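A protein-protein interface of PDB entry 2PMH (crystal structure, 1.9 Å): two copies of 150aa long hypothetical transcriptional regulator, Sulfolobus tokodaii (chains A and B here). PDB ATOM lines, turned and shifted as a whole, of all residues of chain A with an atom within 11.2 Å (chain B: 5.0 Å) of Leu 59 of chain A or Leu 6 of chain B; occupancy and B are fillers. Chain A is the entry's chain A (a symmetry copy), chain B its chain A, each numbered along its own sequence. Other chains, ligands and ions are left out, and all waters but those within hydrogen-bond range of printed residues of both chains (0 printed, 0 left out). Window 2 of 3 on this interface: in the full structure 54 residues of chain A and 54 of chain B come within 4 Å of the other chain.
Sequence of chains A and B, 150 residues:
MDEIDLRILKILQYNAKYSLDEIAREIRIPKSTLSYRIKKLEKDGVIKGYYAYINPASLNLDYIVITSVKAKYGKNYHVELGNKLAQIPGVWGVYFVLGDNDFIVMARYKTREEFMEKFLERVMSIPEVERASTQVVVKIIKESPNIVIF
NH2 of Arg 108 of chain A is in salt-bridge range of OE1 of Glu 143 of chain A. O of Gly 90 of chain A sits at hydrogen-bond distance from N of Arg 108 of chain A, 3.0 Å away.
CB of Leu 9 of chain B touches CD1 of Ile 54 of chain A, at 3.8 Å. Val 148 of chain B touches Ile 54 of chain A (CG2 to CD1, 3.8 Å). Leu 6 of chain B touches Leu 59 of chain A (CD2 to CD2, 3.96 Å). CD1 of Leu 59 of chain A touches CG2 of Val 148 of chain B, at 3.2 Å. CD1 of Leu 59 of chain A touches CG1 of Ile 149 of chain B, at 3.9 Å. NH1 of Arg 108 of chain A touches CG1 of Val 148 of chain B (3.7 Å).
Of the printed residues of chain B, Ile 54 of chain A touches Leu 9 and Val 148. Leu 59 of chain A touches just these residues of chain B: Leu 6, Val 148 and Ile 149. Of the printed residues of chain B, Arg 108 of chain A touches Val 148. No residue of chain A comes within 4 Å of Asp 2 of chain B. Asp 5 of chain B touches none of the printed residues of chain A. Leu 6 of chain B touches just one residue of chain A: Leu 59 (3.96 Å). No residue of chain A comes within 4 Å of Ile 8 of chain B. Leu 9 of chain B touches just one residue of chain A: Ile 54. Val 148 of chain B touches just these residues of chain A: Ile 54, Leu 59 and Arg 108. Printed residues of chain A within 4 Å of Ile 149 of chain B: Leu 59. The nearest residue of chain B that does not touch Leu 59 of chain A is Met 1 of chain B (4.5 Å). The nearest residue of chain A that does not touch Leu 6 of chain B is Ser 58 of chain A (6.5 Å).
Of the 22 printed residues of chain A, 3 touch a printed residue of chain B. Printed residues of chain A that touch a printed residue of chain B: Ile 54, Leu 59 and Arg 108. Of the 12 printed residues of chain B, 4 touch a printed residue of chain A. Printed residues of chain B that touch a printed residue of chain A: Leu 6, Leu 9, Val 148 and Ile 149. Among the printed residues, no Asp or Glu carboxylate lies within 4 Å of a Lys or Arg side-chain nitrogen of the other chain.
No position is printed for both chains. Of the 6 pairs that touch across the chains among the printed residues, none has its exchanged pair printed and touching as well.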
ATOM      1  N   ALA A  52      19.297  -8.378  21.586  1.00  0.00           N
ATOM      2  CA  ALA A  52      18.923  -8.426  20.182  1.00  0.00           C
ATOM      3  C   ALA A  52      18.981  -6.974  19.708  1.00  0.00           C
ATOM      4  O   ALA A  52      18.443  -6.086  20.365  1.00  0.00           O
ATOM      5  CB  ALA A  52      17.512  -8.966  20.028  1.00  0.00           C
ATOM      6  N   TYR A  53      19.653  -6.732  18.589  1.00  0.00           N
ATOM      7  CA  TYR A  53      19.743  -5.382  18.039  1.00  0.00           C
ATOM      8  C   TYR A  53      18.538  -5.145  17.131  1.00  0.00           C
ATOM      9  O   TYR A  53      18.462  -5.683  16.028  1.00  0.00           O
ATOM     10  CB  TYR A  53      21.051  -5.213  17.257  1.00  0.00           C
ATOM     11  CG  TYR A  53      21.121  -3.954  16.420  1.00  0.00           C
ATOM     12  CD1 TYR A  53      20.816  -2.703  16.964  1.00  0.00           C
ATOM     13  CD2 TYR A  53      21.491  -4.014  15.079  1.00  0.00           C
ATOM     14  CE1 TYR A  53      20.876  -1.539  16.184  1.00  0.00           C
ATOM     15  CE2 TYR A  53      21.555  -2.863  14.291  1.00  0.00           C
ATOM     16  CZ  TYR A  53      21.246  -1.631  14.846  1.00  0.00           C
ATOM     17  OH  TYR A  53      21.299  -0.504  14.053  1.00  0.00           O
ATOM     18  N   ILE A  54      17.594  -4.346  17.618  1.00  0.00           N
ATOM     19  CA  ILE A  54      16.374  -4.032  16.885  1.00  0.00           C
ATOM     20  C   ILE A  54      16.508  -2.717  16.132  1.00  0.00           C
ATOM     21  O   ILE A  54      16.960  -1.715  16.688  1.00  0.00           O
ATOM     22  CB  ILE A  54      15.172  -3.914  17.849  1.00  0.00           C
ATOM     23  CG1 ILE A  54      14.984  -5.232  18.603  1.00  0.00           C
ATOM     24  CG2 ILE A  54      13.905  -3.525  17.078  1.00  0.00           C
ATOM     25  CD1 ILE A  54      13.958  -5.150  19.687  1.00  0.00           C
ATOM     26  N   ASN A  55      16.112  -2.735  14.863  1.00  0.00           N
ATOM     27  CA  ASN A  55      16.163  -1.550  14.018  1.00  0.00           C
ATOM     28  C   ASN A  55      15.058  -0.581  14.450  1.00  0.00           C
ATOM     29  O   ASN A  55      13.874  -0.880  14.326  1.00  0.00           O
ATOM     30  CB  ASN A  55      15.985  -1.954  12.552  1.00  0.00           C
ATOM     31  CG  ASN A  55      15.934  -0.757  11.619  1.00  0.00           C
ATOM     32  OD1 ASN A  55      16.774   0.146  11.697  1.00  0.00           O
ATOM     33  ND2 ASN A  55      14.949  -0.746  10.726  1.00  0.00           N
ATOM     34  N   PRO A  56      15.441   0.588  14.990  1.00  0.00           N
ATOM     35  CA  PRO A  56      14.513   1.622  15.458  1.00  0.00           C
ATOM     36  C   PRO A  56      13.446   2.009  14.441  1.00  0.00           C
ATOM     37  O   PRO A  56      12.308   2.302  14.809  1.00  0.00           O
ATOM     38  CB  PRO A  56      15.444   2.782  15.797  1.00  0.00           C
ATOM     39  CG  PRO A  56      16.663   2.074  16.296  1.00  0.00           C
ATOM     40  CD  PRO A  56      16.834   0.990  15.251  1.00  0.00           C
ATOM     41  N   ALA A  57      13.815   2.008  13.165  1.00  0.00           N
ATOM     42  CA  ALA A  57      12.878   2.355  12.102  1.00  0.00           C
ATOM     43  C   ALA A  57      11.740   1.350  12.075  1.00  0.00           C
ATOM     44  O   ALA A  57      10.588   1.703  11.822  1.00  0.00           O
ATOM     45  CB  ALA A  57      13.592   2.363  10.765  1.00  0.00           C
ATOM     46  N   SER A  58      12.078   0.094  12.344  1.00  0.00           N
ATOM     47  CA  SER A  58      11.098  -0.981  12.361  1.00  0.00           C
ATOM     48  C   SER A  58      10.045  -0.701  13.417  1.00  0.00           C
ATOM     49  O   SER A  58       8.942  -1.241  13.365  1.00  0.00           O
ATOM     50  CB  SER A  58      11.780  -2.314  12.654  1.00  0.00           C
ATOM     51  OG  SER A  58      12.804  -2.558  11.707  1.00  0.00           O
ATOM     52  N   LEU A  59      10.385   0.148  14.380  1.00  0.00           N
ATOM     53  CA  LEU A  59       9.440   0.495  15.432  1.00  0.00           C
ATOM     54  C   LEU A  59       8.880   1.903  15.229  1.00  0.00           C
ATOM     55  O   LEU A  59       8.238   2.464  16.120  1.00  0.00           O
ATOM     56  CB  LEU A  59      10.123   0.381  16.792  1.00  0.00           C
ATOM     57  CG  LEU A  59      10.556  -1.042  17.141  1.00  0.00           C
ATOM     58  CD1 LEU A  59      11.558  -1.027  18.278  1.00  0.00           C
ATOM     59  CD2 LEU A  59       9.324  -1.855  17.506  1.00  0.00           C
ATOM     60  N   ASN A  60       9.125   2.465  14.047  1.00  0.00           N
ATOM     61  CA  ASN A  60       8.650   3.806  13.695  1.00  0.00           C
ATOM     62  C   ASN A  60       9.219   4.906  14.590  1.00  0.00           C
ATOM     63  O   ASN A  60       8.588   5.940  14.779  1.00  0.00           O
ATOM     64  CB  ASN A  60       7.120   3.853  13.753  1.00  0.00           C
ATOM     65  CG  ASN A  60       6.469   3.111  12.596  1.00  0.00           C
ATOM     66  OD1 ASN A  60       5.378   2.554  12.734  1.00  0.00           O
ATOM     67  ND2 ASN A  60       7.130   3.119  11.440  1.00  0.00           N
ATOM     68  N   LEU A  61      10.401   4.670  15.153  1.00  0.00           N
ATOM     69  CA  LEU A  61      11.052   5.659  16.015  1.00  0.00           C
ATOM     70  C   LEU A  61      11.725   6.660  15.078  1.00  0.00           C
ATOM     71  O   LEU A  61      12.905   6.547  14.754  1.00  0.00           O
ATOM     72  CB  LEU A  61      12.083   4.975  16.913  1.00  0.00           C
ATOM     73  CG  LEU A  61      11.514   3.975  17.920  1.00  0.00           C
ATOM     74  CD1 LEU A  61      12.655   3.203  18.577  1.00  0.00           C
ATOM     75  CD2 LEU A  61      10.676   4.711  18.951  1.00  0.00           C
ATOM     76  N   ASP A  62      10.941   7.645  14.659  1.00  0.00           N
ATOM     77  CA  ASP A  62      11.378   8.654  13.706  1.00  0.00           C
ATOM     78  C   ASP A  62      11.765  10.012  14.290  1.00  0.00           C
ATOM     79  O   ASP A  62      12.358  10.842  13.597  1.00  0.00           O
ATOM     80  CB  ASP A  62      10.262   8.825  12.671  1.00  0.00           C
ATOM     81  CG  ASP A  62      10.698   9.604  11.466  1.00  0.00           C
ATOM     82  OD1 ASP A  62      10.182  10.722  11.271  1.00  0.00           O
ATOM     83  OD2 ASP A  62      11.554   9.101  10.712  1.00  0.00           O
ATOM     84  N   TYR A  63      11.419  10.243  15.550  1.00  0.00           N
ATOM     85  CA  TYR A  63      11.733  11.511  16.198  1.00  0.00           C
ATOM     86  C   TYR A  63      12.831  11.258  17.220  1.00  0.00           C
ATOM     87  O   TYR A  63      12.556  10.900  18.363  1.00  0.00           O
ATOM     88  CB  TYR A  63      10.486  12.064  16.884  1.00  0.00           C
ATOM     89  CG  TYR A  63      10.368  13.567  16.778  1.00  0.00           C
ATOM     90  CD1 TYR A  63       9.910  14.164  15.602  1.00  0.00           C
ATOM     91  CD2 TYR A  63      10.739  14.394  17.841  1.00  0.00           C
ATOM     92  CE1 TYR A  63       9.822  15.550  15.484  1.00  0.00           C
ATOM     93  CE2 TYR A  63      10.659  15.788  17.731  1.00  0.00           C
ATOM     94  CZ  TYR A  63      10.196  16.352  16.547  1.00  0.00           C
ATOM     95  OH  TYR A  63      10.102  17.717  16.427  1.00  0.00           O
ATOM     96  N   ILE A  64      14.075  11.438  16.789  1.00  0.00           N
ATOM     97  CA  ILE A  64      15.240  11.190  17.628  1.00  0.00           C
ATOM     98  C   ILE A  64      15.796  12.514  18.142  1.00  0.00           C
ATOM     99  O   ILE A  64      16.056  13.421  17.354  1.00  0.00           O
ATOM    100  CB  ILE A  64      16.332  10.457  16.812  1.00  0.00           C
ATOM    101  CG1 ILE A  64      15.730   9.233  16.103  1.00  0.00           C
ATOM    102  CG2 ILE A  64      17.494  10.077  17.721  1.00  0.00           C
ATOM    103  CD1 ILE A  64      15.006   8.277  17.022  1.00  0.00           C
ATOM    104  N   GLY A  90      11.436   6.402  26.878  1.00  0.00           N
ATOM    105  CA  GLY A  90      12.030   6.866  25.632  1.00  0.00           C
ATOM    106  C   GLY A  90      13.482   7.300  25.775  1.00  0.00           C
ATOM    107  O   GLY A  90      14.235   7.305  24.801  1.00  0.00           O
ATOM    108  N   TRP A  92      17.160   6.705  26.615  1.00  0.00           N
ATOM    109  CA  TRP A  92      18.079   5.577  26.765  1.00  0.00           C
ATOM    110  C   TRP A  92      19.465   6.003  27.244  1.00  0.00           C
ATOM    111  O   TRP A  92      20.259   5.175  27.694  1.00  0.00           O
ATOM    112  CB  TRP A  92      18.207   4.784  25.459  1.00  0.00           C
ATOM    113  CG  TRP A  92      18.755   5.555  24.285  1.00  0.00           C
ATOM    114  CD1 TRP A  92      18.032   6.153  23.289  1.00  0.00           C
ATOM    115  CD2 TRP A  92      20.139   5.772  23.962  1.00  0.00           C
ATOM    116  NE1 TRP A  92      18.875   6.722  22.365  1.00  0.00           N
ATOM    117  CE2 TRP A  92      20.172   6.503  22.749  1.00  0.00           C
ATOM    118  CE3 TRP A  92      21.354   5.424  24.574  1.00  0.00           C
ATOM    119  CZ2 TRP A  92      21.377   6.885  22.134  1.00  0.00           C
ATOM    120  CZ3 TRP A  92      22.550   5.806  23.963  1.00  0.00           C
ATOM    121  CH2 TRP A  92      22.549   6.529  22.753  1.00  0.00           C
ATOM    122  N   ARG A 108      14.345   8.583  22.079  1.00  0.00           N
ATOM    123  CA  ARG A 108      13.761   8.235  20.791  1.00  0.00           C
ATOM    124  C   ARG A 108      12.255   8.139  20.946  1.00  0.00           C
ATOM    125  O   ARG A 108      11.762   7.571  21.929  1.00  0.00           O
ATOM    126  CB  ARG A 108      14.254   6.875  20.298  1.00  0.00           C
ATOM    127  CG  ARG A 108      15.718   6.569  20.458  1.00  0.00           C
ATOM    128  CD  ARG A 108      16.038   5.357  19.585  1.00  0.00           C
ATOM    129  NE  ARG A 108      17.344   4.749  19.826  1.00  0.00           N
ATOM    130  CZ  ARG A 108      17.611   3.882  20.799  1.00  0.00           C
ATOM    131  NH1 ARG A 108      16.666   3.507  21.655  1.00  0.00           N
ATOM    132  NH2 ARG A 108      18.825   3.363  20.896  1.00  0.00           N
ATOM    133  N   TYR A 109      11.535   8.685  19.973  1.00  0.00           N
ATOM    134  CA  TYR A 109      10.076   8.645  19.960  1.00  0.00           C
ATOM    135  C   TYR A 109       9.617   8.409  18.531  1.00  0.00           C
ATOM    136  O   TYR A 109      10.381   8.618  17.585  1.00  0.00           O
ATOM    137  CB  TYR A 109       9.494   9.955  20.501  1.00  0.00           C
ATOM    138  CG  TYR A 109       9.892  10.190  21.932  1.00  0.00           C
ATOM    139  CD1 TYR A 109       9.294   9.467  22.963  1.00  0.00           C
ATOM    140  CD2 TYR A 109      10.956  11.025  22.245  1.00  0.00           C
ATOM    141  CE1 TYR A 109       9.754   9.557  24.260  1.00  0.00           C
ATOM    142  CE2 TYR A 109      11.429  11.122  23.540  1.00  0.00           C
ATOM    143  CZ  TYR A 109      10.834  10.383  24.542  1.00  0.00           C
ATOM    144  OH  TYR A 109      11.369  10.401  25.804  1.00  0.00           O
ATOM    145  N   LYS A 110       8.378   7.957  18.377  1.00  0.00           N
ATOM    146  CA  LYS A 110       7.844   7.699  17.055  1.00  0.00           C
ATOM    147  C   LYS A 110       7.490   8.990  16.330  1.00  0.00           C
ATOM    148  O   LYS A 110       7.680   9.097  15.127  1.00  0.00           O
ATOM    149  CB  LYS A 110       6.608   6.804  17.143  1.00  0.00           C
ATOM    150  CG  LYS A 110       6.888   5.407  17.667  1.00  0.00           C
ATOM    151  CD  LYS A 110       5.709   4.478  17.429  1.00  0.00           C
ATOM    152  CE  LYS A 110       4.465   4.992  18.123  1.00  0.00           C
ATOM    153  NZ  LYS A 110       4.665   5.015  19.595  1.00  0.00           N
ATOM    154  N   THR A 111       6.987   9.974  17.065  1.00  0.00           N
ATOM    155  CA  THR A 111       6.599  11.246  16.451  1.00  0.00           C
ATOM    156  C   THR A 111       6.835  12.441  17.365  1.00  0.00           C
ATOM    157  O   THR A 111       7.204  12.287  18.527  1.00  0.00           O
ATOM    158  CB  THR A 111       5.107  11.260  16.117  1.00  0.00           C
ATOM    159  OG1 THR A 111       4.370  11.111  17.335  1.00  0.00           O
ATOM    160  CG2 THR A 111       4.742  10.132  15.151  1.00  0.00           C
ATOM    161  N   GLU A 114       4.356  12.395  20.448  1.00  0.00           N
ATOM    162  CA  GLU A 114       4.826  11.493  21.492  1.00  0.00           C
ATOM    163  C   GLU A 114       5.992  12.131  22.246  1.00  0.00           C
ATOM    164  O   GLU A 114       6.056  12.066  23.478  1.00  0.00           O
ATOM    165  CB  GLU A 114       5.243  10.165  20.867  1.00  0.00           C
ATOM    166  CG  GLU A 114       5.740   9.131  21.857  1.00  0.00           C
ATOM    167  CD  GLU A 114       5.864   7.754  21.229  1.00  0.00           C
ATOM    168  OE1 GLU A 114       4.822   7.209  20.812  1.00  0.00           O
ATOM    169  OE2 GLU A 114       6.994   7.226  21.145  1.00  0.00           O
ATOM    170  N   LYS A 118       5.446  12.692  26.191  1.00  0.00           N
ATOM    171  CA  LYS A 118       6.272  11.873  27.071  1.00  0.00           C
ATOM    172  C   LYS A 118       7.564  12.511  27.573  1.00  0.00           C
ATOM    173  O   LYS A 118       7.971  12.285  28.717  1.00  0.00           O
ATOM    174  CB  LYS A 118       6.613  10.557  26.376  1.00  0.00           C
ATOM    175  CG  LYS A 118       5.407   9.693  26.068  1.00  0.00           C
ATOM    176  CD  LYS A 118       5.831   8.393  25.414  1.00  0.00           C
ATOM    177  CE  LYS A 118       4.634   7.496  25.140  1.00  0.00           C
ATOM    178  NZ  LYS A 118       5.065   6.282  24.404  1.00  0.00           N
ATOM    179  N   GLU A 143      25.775   4.558  14.720  1.00  0.00           N
ATOM    180  CA  GLU A 143      25.304   4.275  16.074  1.00  0.00           C
ATOM    181  C   GLU A 143      25.561   2.809  16.377  1.00  0.00           C
ATOM    182  O   GLU A 143      24.686   1.966  16.191  1.00  0.00           O
ATOM    183  CB  GLU A 143      23.813   4.581  16.258  1.00  0.00           C
ATOM    184  CG  GLU A 143      23.426   4.571  17.739  1.00  0.00           C
ATOM    185  CD  GLU A 143      21.955   4.818  17.989  1.00  0.00           C
ATOM    186  OE1 GLU A 143      21.162   3.873  17.811  1.00  0.00           O
ATOM    187  OE2 GLU A 143      21.591   5.954  18.374  1.00  0.00           O
ATOM    188  N   MET B   1       4.496  -6.899  11.453  1.00  0.00           N
ATOM    189  CA  MET B   1       4.561  -7.026  12.937  1.00  0.00           C
ATOM    190  C   MET B   1       3.215  -6.851  13.629  1.00  0.00           C
ATOM    191  O   MET B   1       2.433  -5.964  13.280  1.00  0.00           O
ATOM    192  CB  MET B   1       5.538  -6.003  13.512  1.00  0.00           C
ATOM    193  CG  MET B   1       6.999  -6.335  13.306  1.00  0.00           C
ATOM    194  SD  MET B   1       8.010  -5.220  14.290  1.00  0.00           S
ATOM    195  CE  MET B   1       7.314  -5.510  15.910  1.00  0.00           C
ATOM    196  N   ASP B   2       2.963  -7.699  14.623  1.00  0.00           N
ATOM    197  CA  ASP B   2       1.725  -7.659  15.400  1.00  0.00           C
ATOM    198  C   ASP B   2       2.067  -7.546  16.885  1.00  0.00           C
ATOM    199  O   ASP B   2       3.239  -7.577  17.255  1.00  0.00           O
ATOM    200  CB  ASP B   2       0.902  -8.928  15.154  1.00  0.00           C
ATOM    201  CG  ASP B   2       1.706 -10.194  15.376  1.00  0.00           C
ATOM    202  OD1 ASP B   2       2.319 -10.325  16.454  1.00  0.00           O
ATOM    203  OD2 ASP B   2       1.724 -11.060  14.476  1.00  0.00           O
ATOM    204  N   GLU B   3       1.045  -7.426  17.727  1.00  0.00           N
ATOM    205  CA  GLU B   3       1.254  -7.301  19.164  1.00  0.00           C
ATOM    206  C   GLU B   3       2.109  -8.433  19.733  1.00  0.00           C
ATOM    207  O   GLU B   3       2.798  -8.250  20.736  1.00  0.00           O
ATOM    208  CB  GLU B   3      -0.088  -7.261  19.896  1.00  0.00           C
ATOM    209  CG  GLU B   3      -1.082  -6.250  19.332  1.00  0.00           C
ATOM    210  CD  GLU B   3      -2.282  -6.027  20.254  1.00  0.00           C
ATOM    211  OE1 GLU B   3      -2.827  -7.026  20.782  1.00  0.00           O
ATOM    212  OE2 GLU B   3      -2.682  -4.852  20.440  1.00  0.00           O
ATOM    213  N   ILE B   4       2.065  -9.602  19.098  1.00  0.00           N
ATOM    214  CA  ILE B   4       2.854 -10.740  19.561  1.00  0.00           C
ATOM    215  C   ILE B   4       4.346 -10.512  19.310  1.00  0.00           C
ATOM    216  O   ILE B   4       5.180 -10.843  20.153  1.00  0.00           O
ATOM    217  CB  ILE B   4       2.429 -12.059  18.861  1.00  0.00           C
ATOM    218  CG1 ILE B   4       1.048 -12.496  19.356  1.00  0.00           C
ATOM    219  CG2 ILE B   4       3.459 -13.155  19.136  1.00  0.00           C
ATOM    220  CD1 ILE B   4       0.999 -12.808  20.837  1.00  0.00           C
ATOM    221  N   ASP B   5       4.677  -9.959  18.146  1.00  0.00           N
ATOM    222  CA  ASP B   5       6.070  -9.689  17.810  1.00  0.00           C
ATOM    223  C   ASP B   5       6.670  -8.695  18.804  1.00  0.00           C
ATOM    224  O   ASP B   5       7.807  -8.856  19.245  1.00  0.00           O
ATOM    225  CB  ASP B   5       6.180  -9.134  16.389  1.00  0.00           C
ATOM    226  CG  ASP B   5       5.818 -10.161  15.335  1.00  0.00           C
ATOM    227  OD1 ASP B   5       6.346 -11.291  15.397  1.00  0.00           O
ATOM    228  OD2 ASP B   5       5.014  -9.833  14.440  1.00  0.00           O
ATOM    229  N   LEU B   6       5.896  -7.672  19.154  1.00  0.00           N
ATOM    230  CA  LEU B   6       6.341  -6.658  20.103  1.00  0.00           C
ATOM    231  C   LEU B   6       6.678  -7.260  21.464  1.00  0.00           C
ATOM    232  O   LEU B   6       7.646  -6.851  22.113  1.00  0.00           O
ATOM    233  CB  LEU B   6       5.261  -5.594  20.281  1.00  0.00           C
ATOM    234  CG  LEU B   6       4.948  -4.761  19.042  1.00  0.00           C
ATOM    235  CD1 LEU B   6       3.831  -3.772  19.364  1.00  0.00           C
ATOM    236  CD2 LEU B   6       6.203  -4.030  18.590  1.00  0.00           C
ATOM    237  N   ARG B   7       5.867  -8.224  21.897  1.00  0.00           N
ATOM    238  CA  ARG B   7       6.078  -8.894  23.176  1.00  0.00           C
ATOM    239  C   ARG B   7       7.365  -9.710  23.098  1.00  0.00           C
ATOM    240  O   ARG B   7       8.115  -9.792  24.069  1.00  0.00           O
ATOM    241  CB  ARG B   7       4.894  -9.818  23.496  1.00  0.00           C
ATOM    242  CG  ARG B   7       3.544  -9.110  23.540  1.00  0.00           C
ATOM    243  CD  ARG B   7       2.930  -9.139  24.938  1.00  0.00           C
ATOM    244  NE  ARG B   7       2.713 -10.504  25.424  1.00  0.00           N
ATOM    245  CZ  ARG B   7       1.926 -11.404  24.835  1.00  0.00           C
ATOM    246  NH1 ARG B   7       1.263 -11.096  23.725  1.00  0.00           N
ATOM    247  NH2 ARG B   7       1.804 -12.619  25.359  1.00  0.00           N
ATOM    248  N   ILE B   8       7.606 -10.324  21.943  1.00  0.00           N
ATOM    249  CA  ILE B   8       8.814 -11.116  21.744  1.00  0.00           C
ATOM    250  C   ILE B   8      10.016 -10.172  21.775  1.00  0.00           C
ATOM    251  O   ILE B   8      10.995 -10.412  22.480  1.00  0.00           O
ATOM    252  CB  ILE B   8       8.798 -11.844  20.387  1.00  0.00           C
ATOM    253  CG1 ILE B   8       7.664 -12.873  20.354  1.00  0.00           C
ATOM    254  CG2 ILE B   8      10.139 -12.533  20.146  1.00  0.00           C
ATOM    255  CD1 ILE B   8       7.558 -13.607  19.023  1.00  0.00           C
ATOM    256  N   LEU B   9       9.927  -9.093  21.007  1.00  0.00           N
ATOM    257  CA  LEU B   9      11.005  -8.116  20.944  1.00  0.00           C
ATOM    258  C   LEU B   9      11.291  -7.474  22.299  1.00  0.00           C
ATOM    259  O   LEU B   9      12.452  -7.241  22.642  1.00  0.00           O
ATOM    260  CB  LEU B   9      10.673  -7.034  19.907  1.00  0.00           C
ATOM    261  CG  LEU B   9      10.643  -7.506  18.447  1.00  0.00           C
ATOM    262  CD1 LEU B   9      10.208  -6.368  17.538  1.00  0.00           C
ATOM    263  CD2 LEU B   9      12.016  -8.031  18.039  1.00  0.00           C
ATOM    264  N   LYS B  10      10.244  -7.203  23.076  1.00  0.00           N
ATOM    265  CA  LYS B  10      10.426  -6.574  24.382  1.00  0.00           C
ATOM    266  C   LYS B  10      11.250  -7.458  25.314  1.00  0.00           C
ATOM    267  O   LYS B  10      11.795  -6.984  26.314  1.00  0.00           O
ATOM    268  CB  LYS B  10       9.073  -6.246  25.020  1.00  0.00           C
ATOM    269  CG  LYS B  10       9.178  -5.352  26.250  1.00  0.00           C
ATOM    270  CD  LYS B  10       7.820  -4.780  26.614  1.00  0.00           C
ATOM    271  CE  LYS B  10       7.909  -3.841  27.805  1.00  0.00           C
ATOM    272  NZ  LYS B  10       6.605  -3.188  28.094  1.00  0.00           N
ATOM    273  N   VAL B 148      14.522  -0.346  23.133  1.00  0.00           N
ATOM    274  CA  VAL B 148      13.764   0.447  22.172  1.00  0.00           C
ATOM    275  C   VAL B 148      12.265   0.376  22.462  1.00  0.00           C
ATOM    276  O   VAL B 148      11.495   1.219  22.001  1.00  0.00           O
ATOM    277  CB  VAL B 148      14.029  -0.031  20.721  1.00  0.00           C
ATOM    278  CG1 VAL B 148      15.483   0.247  20.337  1.00  0.00           C
ATOM    279  CG2 VAL B 148      13.725  -1.521  20.603  1.00  0.00           C
ATOM    280  N   ILE B 149      11.857  -0.630  23.235  1.00  0.00           N
ATOM    281  CA  ILE B 149      10.454  -0.804  23.600  1.00  0.00           C
ATOM    282  C   ILE B 149      10.319  -0.608  25.117  1.00  0.00           C
ATOM    283  O   ILE B 149      10.772  -1.439  25.911  1.00  0.00           O
ATOM    284  CB  ILE B 149       9.961  -2.212  23.174  1.00  0.00           C
ATOM    285  CG1 ILE B 149      10.148  -2.379  21.666  1.00  0.00           C
ATOM    286  CG2 ILE B 149       8.490  -2.396  23.530  1.00  0.00           C
ATOM    287  CD1 ILE B 149       9.970  -3.800  21.165  1.00  0.00           C
